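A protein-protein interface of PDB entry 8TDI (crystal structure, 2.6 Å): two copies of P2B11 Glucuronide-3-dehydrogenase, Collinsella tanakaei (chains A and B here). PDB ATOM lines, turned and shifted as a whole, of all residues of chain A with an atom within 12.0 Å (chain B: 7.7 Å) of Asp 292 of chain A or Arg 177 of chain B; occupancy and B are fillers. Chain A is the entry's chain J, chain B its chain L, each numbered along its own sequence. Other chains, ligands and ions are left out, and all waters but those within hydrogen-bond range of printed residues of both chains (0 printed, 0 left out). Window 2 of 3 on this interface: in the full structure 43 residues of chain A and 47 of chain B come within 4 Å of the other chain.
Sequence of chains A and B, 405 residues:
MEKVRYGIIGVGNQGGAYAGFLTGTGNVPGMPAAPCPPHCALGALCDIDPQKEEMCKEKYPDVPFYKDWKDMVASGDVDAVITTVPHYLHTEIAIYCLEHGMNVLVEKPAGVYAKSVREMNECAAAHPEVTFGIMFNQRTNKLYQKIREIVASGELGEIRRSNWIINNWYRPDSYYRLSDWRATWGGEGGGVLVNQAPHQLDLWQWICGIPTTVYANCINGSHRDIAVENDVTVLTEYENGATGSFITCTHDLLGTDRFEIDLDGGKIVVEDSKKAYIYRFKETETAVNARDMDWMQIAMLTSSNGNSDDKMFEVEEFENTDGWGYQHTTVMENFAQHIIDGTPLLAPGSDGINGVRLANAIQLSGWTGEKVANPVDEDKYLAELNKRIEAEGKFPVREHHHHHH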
ATOM      1  N   GLU A 283      10.041  -0.315  -7.530  1.00  0.00           N
ATOM      2  CA  GLU A 283      10.813  -1.033  -8.525  1.00  0.00           C
ATOM      3  C   GLU A 283      12.092  -1.517  -7.873  1.00  0.00           C
ATOM      4  O   GLU A 283      12.585  -0.864  -6.953  1.00  0.00           O
ATOM      5  CB  GLU A 283      11.144  -0.103  -9.691  1.00  0.00           C
ATOM      6  CG  GLU A 283      10.310  -0.399 -10.927  1.00  0.00           C
ATOM      7  CD  GLU A 283      10.409   0.700 -11.976  1.00  0.00           C
ATOM      8  OE1 GLU A 283      10.190   0.373 -13.158  1.00  0.00           O
ATOM      9  OE2 GLU A 283      10.753   1.867 -11.641  1.00  0.00           O
ATOM     10  N   THR A 284      12.638  -2.620  -8.386  1.00  0.00           N
ATOM     11  CA  THR A 284      13.888  -3.141  -7.853  1.00  0.00           C
ATOM     12  C   THR A 284      15.000  -2.153  -8.189  1.00  0.00           C
ATOM     13  O   THR A 284      14.927  -1.451  -9.194  1.00  0.00           O
ATOM     14  CB  THR A 284      14.200  -4.520  -8.432  1.00  0.00           C
ATOM     15  OG1 THR A 284      14.783  -4.273  -9.699  1.00  0.00           O
ATOM     16  CG2 THR A 284      12.981  -5.412  -8.605  1.00  0.00           C
ATOM     17  N   GLU A 285      16.045  -2.123  -7.357  1.00  0.00           N
ATOM     18  CA  GLU A 285      17.156  -1.224  -7.591  1.00  0.00           C
ATOM     19  C   GLU A 285      17.773  -1.545  -8.949  1.00  0.00           C
ATOM     20  O   GLU A 285      18.142  -0.642  -9.682  1.00  0.00           O
ATOM     21  CB  GLU A 285      18.181  -1.332  -6.468  1.00  0.00           C
ATOM     22  CG  GLU A 285      19.258  -0.256  -6.514  1.00  0.00           C
ATOM     23  CD  GLU A 285      20.410  -0.461  -7.488  1.00  0.00           C
ATOM     24  OE1 GLU A 285      20.831   0.565  -8.038  1.00  0.00           O
ATOM     25  OE2 GLU A 285      20.878  -1.605  -7.684  1.00  0.00           O
ATOM     26  N   THR A 286      17.866  -2.840  -9.272  1.00  0.00           N
ATOM     27  CA  THR A 286      18.429  -3.264 -10.545  1.00  0.00           C
ATOM     28  C   THR A 286      17.682  -2.567 -11.676  1.00  0.00           C
ATOM     29  O   THR A 286      18.303  -2.036 -12.587  1.00  0.00           O
ATOM     30  CB  THR A 286      18.363  -4.785 -10.687  1.00  0.00           C
ATOM     31  OG1 THR A 286      18.878  -5.259  -9.447  1.00  0.00           O
ATOM     32  CG2 THR A 286      19.134  -5.307 -11.888  1.00  0.00           C
ATOM     33  N   ALA A 287      16.348  -2.551 -11.579  1.00  0.00           N
ATOM     34  CA  ALA A 287      15.505  -1.885 -12.561  1.00  0.00           C
ATOM     35  C   ALA A 287      15.789  -0.381 -12.604  1.00  0.00           C
ATOM     36  O   ALA A 287      15.905   0.206 -13.685  1.00  0.00           O
ATOM     37  CB  ALA A 287      14.050  -2.159 -12.253  1.00  0.00           C
ATOM     38  N   VAL A 288      15.898   0.242 -11.426  1.00  0.00           N
ATOM     39  CA  VAL A 288      16.131   1.676 -11.339  1.00  0.00           C
ATOM     40  C   VAL A 288      17.473   2.009 -11.993  1.00  0.00           C
ATOM     41  O   VAL A 288      17.583   2.978 -12.750  1.00  0.00           O
ATOM     42  CB  VAL A 288      16.062   2.173  -9.884  1.00  0.00           C
ATOM     43  CG1 VAL A 288      16.370   3.667  -9.768  1.00  0.00           C
ATOM     44  CG2 VAL A 288      14.706   1.863  -9.249  1.00  0.00           C
ATOM     45  N   ASN A 289      18.490   1.186 -11.705  1.00  0.00           N
ATOM     46  CA  ASN A 289      19.833   1.416 -12.209  1.00  0.00           C
ATOM     47  C   ASN A 289      19.819   1.320 -13.733  1.00  0.00           C
ATOM     48  O   ASN A 289      20.507   2.085 -14.400  1.00  0.00           O
ATOM     49  CB  ASN A 289      20.820   0.447 -11.562  1.00  0.00           C
ATOM     50  CG  ASN A 289      22.252   0.820 -11.811  1.00  0.00           C
ATOM     51  OD1 ASN A 289      22.564   2.018 -11.836  1.00  0.00           O
ATOM     52  ND2 ASN A 289      23.100  -0.182 -12.025  1.00  0.00           N
ATOM     53  N   ALA A 290      19.024   0.375 -14.260  1.00  0.00           N
ATOM     54  CA  ALA A 290      18.932   0.130 -15.689  1.00  0.00           C
ATOM     55  C   ALA A 290      18.330   1.334 -16.426  1.00  0.00           C
ATOM     56  O   ALA A 290      18.678   1.555 -17.582  1.00  0.00           O
ATOM     57  CB  ALA A 290      18.129  -1.126 -15.934  1.00  0.00           C
ATOM     58  N   ARG A 291      17.455   2.093 -15.762  1.00  0.00           N
ATOM     59  CA  ARG A 291      16.681   3.129 -16.434  1.00  0.00           C
ATOM     60  C   ARG A 291      17.555   4.273 -16.959  1.00  0.00           C
ATOM     61  O   ARG A 291      17.258   4.875 -17.997  1.00  0.00           O
ATOM     62  CB  ARG A 291      15.598   3.770 -15.580  1.00  0.00           C
ATOM     63  CG  ARG A 291      14.416   4.354 -16.343  1.00  0.00           C
ATOM     64  CD  ARG A 291      13.134   4.258 -15.516  1.00  0.00           C
ATOM     65  NE  ARG A 291      12.956   2.944 -14.889  1.00  0.00           N
ATOM     66  CZ  ARG A 291      13.122   2.697 -13.604  1.00  0.00           C
ATOM     67  NH1 ARG A 291      13.065   3.658 -12.693  1.00  0.00           N
ATOM     68  NH2 ARG A 291      13.269   1.447 -13.242  1.00  0.00           N
ATOM     69  N   ASP A 292      18.563   4.704 -16.192  1.00  0.00           N
ATOM     70  CA  ASP A 292      19.437   5.787 -16.622  1.00  0.00           C
ATOM     71  C   ASP A 292      18.576   7.034 -16.852  1.00  0.00           C
ATOM     72  O   ASP A 292      19.103   8.126 -16.675  1.00  0.00           O
ATOM     73  CB  ASP A 292      20.210   5.391 -17.876  1.00  0.00           C
ATOM     74  CG  ASP A 292      20.758   3.972 -17.886  1.00  0.00           C
ATOM     75  OD1 ASP A 292      21.366   3.573 -16.859  1.00  0.00           O
ATOM     76  OD2 ASP A 292      20.537   3.273 -18.907  1.00  0.00           O
ATOM     77  N   PRO B 172      23.550   5.791  -9.183  1.00  0.00           N
ATOM     78  CA  PRO B 172      23.421   4.806 -10.257  1.00  0.00           C
ATOM     79  C   PRO B 172      24.514   4.913 -11.313  1.00  0.00           C
ATOM     80  O   PRO B 172      25.270   5.878 -11.346  1.00  0.00           O
ATOM     81  CB  PRO B 172      22.050   5.142 -10.826  1.00  0.00           C
ATOM     82  CG  PRO B 172      21.955   6.646 -10.653  1.00  0.00           C
ATOM     83  CD  PRO B 172      22.645   6.939  -9.340  1.00  0.00           C
ATOM     84  N   ASP B 173      24.550   3.916 -12.190  1.00  0.00           N
ATOM     85  CA  ASP B 173      25.520   3.835 -13.273  1.00  0.00           C
ATOM     86  C   ASP B 173      25.581   5.157 -14.039  1.00  0.00           C
ATOM     87  O   ASP B 173      26.656   5.604 -14.405  1.00  0.00           O
ATOM     88  CB  ASP B 173      25.265   2.621 -14.156  1.00  0.00           C
ATOM     89  CG  ASP B 173      25.963   1.348 -13.687  1.00  0.00           C
ATOM     90  OD1 ASP B 173      27.128   1.466 -13.260  1.00  0.00           O
ATOM     91  OD2 ASP B 173      25.357   0.248 -13.773  1.00  0.00           O
ATOM     92  N   SER B 174      24.433   5.803 -14.245  1.00  0.00           N
ATOM     93  CA  SER B 174      24.364   7.061 -14.968  1.00  0.00           C
ATOM     94  C   SER B 174      25.244   8.134 -14.321  1.00  0.00           C
ATOM     95  O   SER B 174      25.859   8.909 -15.040  1.00  0.00           O
ATOM     96  CB  SER B 174      22.940   7.566 -15.103  1.00  0.00           C
ATOM     97  OG  SER B 174      21.986   6.895 -14.285  1.00  0.00           O
ATOM     98  N   TYR B 175      25.254   8.217 -12.984  1.00  0.00           N
ATOM     99  CA  TYR B 175      26.110   9.159 -12.273  1.00  0.00           C
ATOM    100  C   TYR B 175      27.578   8.809 -12.512  1.00  0.00           C
ATOM    101  O   TYR B 175      28.413   9.695 -12.668  1.00  0.00           O
ATOM    102  CB  TYR B 175      25.876   9.171 -10.758  1.00  0.00           C
ATOM    103  CG  TYR B 175      26.878   9.915  -9.874  1.00  0.00           C
ATOM    104  CD1 TYR B 175      27.970   9.256  -9.289  1.00  0.00           C
ATOM    105  CD2 TYR B 175      26.695  11.261  -9.555  1.00  0.00           C
ATOM    106  CE1 TYR B 175      28.863   9.923  -8.463  1.00  0.00           C
ATOM    107  CE2 TYR B 175      27.581  11.933  -8.726  1.00  0.00           C
ATOM    108  CZ  TYR B 175      28.668  11.266  -8.182  1.00  0.00           C
ATOM    109  OH  TYR B 175      29.529  11.916  -7.342  1.00  0.00           O
ATOM    110  N   TYR B 176      27.892   7.515 -12.472  1.00  0.00           N
ATOM    111  CA  TYR B 176      29.273   7.074 -12.599  1.00  0.00           C
ATOM    112  C   TYR B 176      29.805   7.461 -13.984  1.00  0.00           C
ATOM    113  O   TYR B 176      30.957   7.856 -14.103  1.00  0.00           O
ATOM    114  CB  TYR B 176      29.424   5.588 -12.249  1.00  0.00           C
ATOM    115  CG  TYR B 176      29.445   5.317 -10.745  1.00  0.00           C
ATOM    116  CD1 TYR B 176      30.565   5.638  -9.985  1.00  0.00           C
ATOM    117  CD2 TYR B 176      28.366   4.726 -10.086  1.00  0.00           C
ATOM    118  CE1 TYR B 176      30.597   5.423  -8.619  1.00  0.00           C
ATOM    119  CE2 TYR B 176      28.391   4.495  -8.721  1.00  0.00           C
ATOM    120  CZ  TYR B 176      29.509   4.847  -7.985  1.00  0.00           C
ATOM    121  OH  TYR B 176      29.560   4.633  -6.643  1.00  0.00           O
ATOM    122  N   ARG B 177      28.946   7.439 -15.009  1.00  0.00           N
ATOM    123  CA  ARG B 177      29.369   7.764 -16.365  1.00  0.00           C
ATOM    124  C   ARG B 177      29.660   9.260 -16.547  1.00  0.00           C
ATOM    125  O   ARG B 177      30.284   9.641 -17.528  1.00  0.00           O
ATOM    126  CB  ARG B 177      28.299   7.297 -17.363  1.00  0.00           C
ATOM    127  CG  ARG B 177      28.203   5.787 -17.453  1.00  0.00           C
ATOM    128  CD  ARG B 177      27.106   5.394 -18.449  1.00  0.00           C
ATOM    129  NE  ARG B 177      25.790   5.362 -17.814  1.00  0.00           N
ATOM    130  CZ  ARG B 177      25.147   4.214 -17.529  1.00  0.00           C
ATOM    131  NH1 ARG B 177      25.785   3.061 -17.564  1.00  0.00           N
ATOM    132  NH2 ARG B 177      23.942   4.197 -17.040  1.00  0.00           N
ATOM    133  N   LEU B 178      29.214  10.107 -15.614  1.00  0.00           N
ATOM    134  CA  LEU B 178      29.353  11.555 -15.765  1.00  0.00           C
ATOM    135  C   LEU B 178      30.816  12.025 -15.796  1.00  0.00           C
ATOM    136  O   LEU B 178      31.132  12.911 -16.587  1.00  0.00           O
ATOM    137  CB  LEU B 178      28.561  12.269 -14.669  1.00  0.00           C
ATOM    138  CG  LEU B 178      27.046  12.037 -14.684  1.00  0.00           C
ATOM    139  CD1 LEU B 178      26.382  12.819 -13.551  1.00  0.00           C
ATOM    140  CD2 LEU B 178      26.431  12.389 -16.027  1.00  0.00           C
ATOM    141  N   SER B 179      31.709  11.473 -14.959  1.00  0.00           N
ATOM    142  CA  SER B 179      33.088  11.960 -14.898  1.00  0.00           C
ATOM    143  C   SER B 179      34.070  10.847 -15.251  1.00  0.00           C
ATOM    144  O   SER B 179      34.019   9.786 -14.646  1.00  0.00           O
ATOM    145  CB  SER B 179      33.445  12.553 -13.534  1.00  0.00           C
ATOM    146  OG  SER B 179      34.794  12.279 -13.185  1.00  0.00           O
ATOM    147  N   ASP B 180      35.003  11.131 -16.181  1.00  0.00           N
ATOM    148  CA  ASP B 180      36.036  10.176 -16.551  1.00  0.00           C
ATOM    149  C   ASP B 180      36.986   9.876 -15.387  1.00  0.00           C
ATOM    150  O   ASP B 180      37.315   8.706 -15.150  1.00  0.00           O
ATOM    151  CB  ASP B 180      36.826  10.669 -17.745  1.00  0.00           C
ATOM    152  CG  ASP B 180      37.291  12.117 -17.677  1.00  0.00           C
ATOM    153  OD1 ASP B 180      38.525  12.315 -17.760  1.00  0.00           O
ATOM    154  OD2 ASP B 180      36.477  13.014 -17.436  1.00  0.00           O
ATOM    155  N   ARG B 182      36.548  10.240 -12.062  1.00  0.00           N
ATOM    156  CA  ARG B 182      35.941   9.615 -10.892  1.00  0.00           C
ATOM    157  C   ARG B 182      35.741   8.115 -11.109  1.00  0.00           C
ATOM    158  O   ARG B 182      35.506   7.702 -12.226  1.00  0.00           O
ATOM    159  CB  ARG B 182      34.635  10.332 -10.514  1.00  0.00           C
ATOM    160  CG  ARG B 182      34.899  11.693  -9.891  1.00  0.00           C
ATOM    161  CD  ARG B 182      34.275  11.813  -8.545  1.00  0.00           C
ATOM    162  NE  ARG B 182      34.327  13.147  -7.962  1.00  0.00           N
ATOM    163  CZ  ARG B 182      34.815  13.505  -6.784  1.00  0.00           C
ATOM    164  NH1 ARG B 182      35.525  12.675  -6.059  1.00  0.00           N
ATOM    165  NH2 ARG B 182      34.641  14.756  -6.396  1.00  0.00           N
ATOM    166  N   ALA B 183      35.866   7.314 -10.035  1.00  0.00           N
ATOM    167  CA  ALA B 183      35.637   5.870 -10.015  1.00  0.00           C
ATOM    168  C   ALA B 183      36.613   5.117 -10.922  1.00  0.00           C
ATOM    169  O   ALA B 183      36.258   4.079 -11.485  1.00  0.00           O
ATOM    170  CB  ALA B 183      34.196   5.591 -10.360  1.00  0.00           C
ATOM    171  N   ASP B 225      28.760  -0.910 -12.933  1.00  0.00           N
ATOM    172  CA  ASP B 225      29.706  -1.197 -13.991  1.00  0.00           C
ATOM    173  C   ASP B 225      30.928  -0.301 -13.806  1.00  0.00           C
ATOM    174  O   ASP B 225      31.194   0.576 -14.630  1.00  0.00           O
ATOM    175  CB  ASP B 225      29.034  -1.003 -15.338  1.00  0.00           C
ATOM    176  CG  ASP B 225      29.920  -1.313 -16.535  1.00  0.00           C
ATOM    177  OD1 ASP B 225      30.983  -1.937 -16.333  1.00  0.00           O
ATOM    178  OD2 ASP B 225      29.562  -0.890 -17.649  1.00  0.00           O
ATOM    179  N   ILE B 226      31.664  -0.543 -12.715  1.00  0.00           N
ATOM    180  CA  ILE B 226      32.892   0.172 -12.407  1.00  0.00           C
ATOM    181  C   ILE B 226      33.883  -0.839 -11.850  1.00  0.00           C
ATOM    182  O   ILE B 226      33.482  -1.914 -11.418  1.00  0.00           O
ATOM    183  CB  ILE B 226      32.635   1.299 -11.393  1.00  0.00           C
ATOM    184  CG1 ILE B 226      32.180   0.726 -10.042  1.00  0.00           C
ATOM    185  CG2 ILE B 226      31.641   2.315 -11.950  1.00  0.00           C
ATOM    186  CD1 ILE B 226      31.737   1.764  -9.026  1.00  0.00           C
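No position is printed for both chains.
Hydrophobic or aromatic side chains of chain B that line the printed part of chain A: Pro 172. Of the 10 printed residues of chain A, 2 touch a printed residue of chain B. Among the printed residues, 4 pairs touch across the chains.
N of Asp 173 of chain B sits at hydrogen-bond distance from OD1 of Asn 289 of chain A. NH2 of Arg 177 of chain B lies within salt-bridge range of OD1 of Asp 292 of chain A.
The backbone NH (N) of Asp 225 of chain B lies within hydrogen-bond range of the side-chain carboxylate (OD1) of Asp 173 of chain B, 2.9 Å away.
OD1 of Asn 289 of chain A touches CA of Pro 172 of chain B, at 3.3 Å. Ser 174 of chain B touches Asp 292 of chain A (OG to CA, 3.6 Å).
Thr 284 of chain A touches none of the printed residues of chain B. Of the printed residues of chain B, Asn 289 of chain A touches Pro 172 and Asp 173. Ala 290 of chain A touches none of the printed residues of chain B. Asp 292 of chain A touches two residues of chain B. Printed residues of chain A within 4 Å of Pro 172 of chain B: Asn 289 (3.3 Å). Of chain A, only Asp 292 comes within 4 Å of Ser 174 of chain B. Of chain A, only Asp 292 comes within 4 Å of Arg 177 of chain B. No residue of chain A comes within 4 Å of Leu 178 of chain B. No residue of chain A comes within 4 Å of Ser 179 of chain B. No residue of chain A comes within 4 Å of Asp 225 of chain B. The nearest printed residue of chain B that does not touch Asn 289 of chain A is Arg 177 of chain B (4.8 Å).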
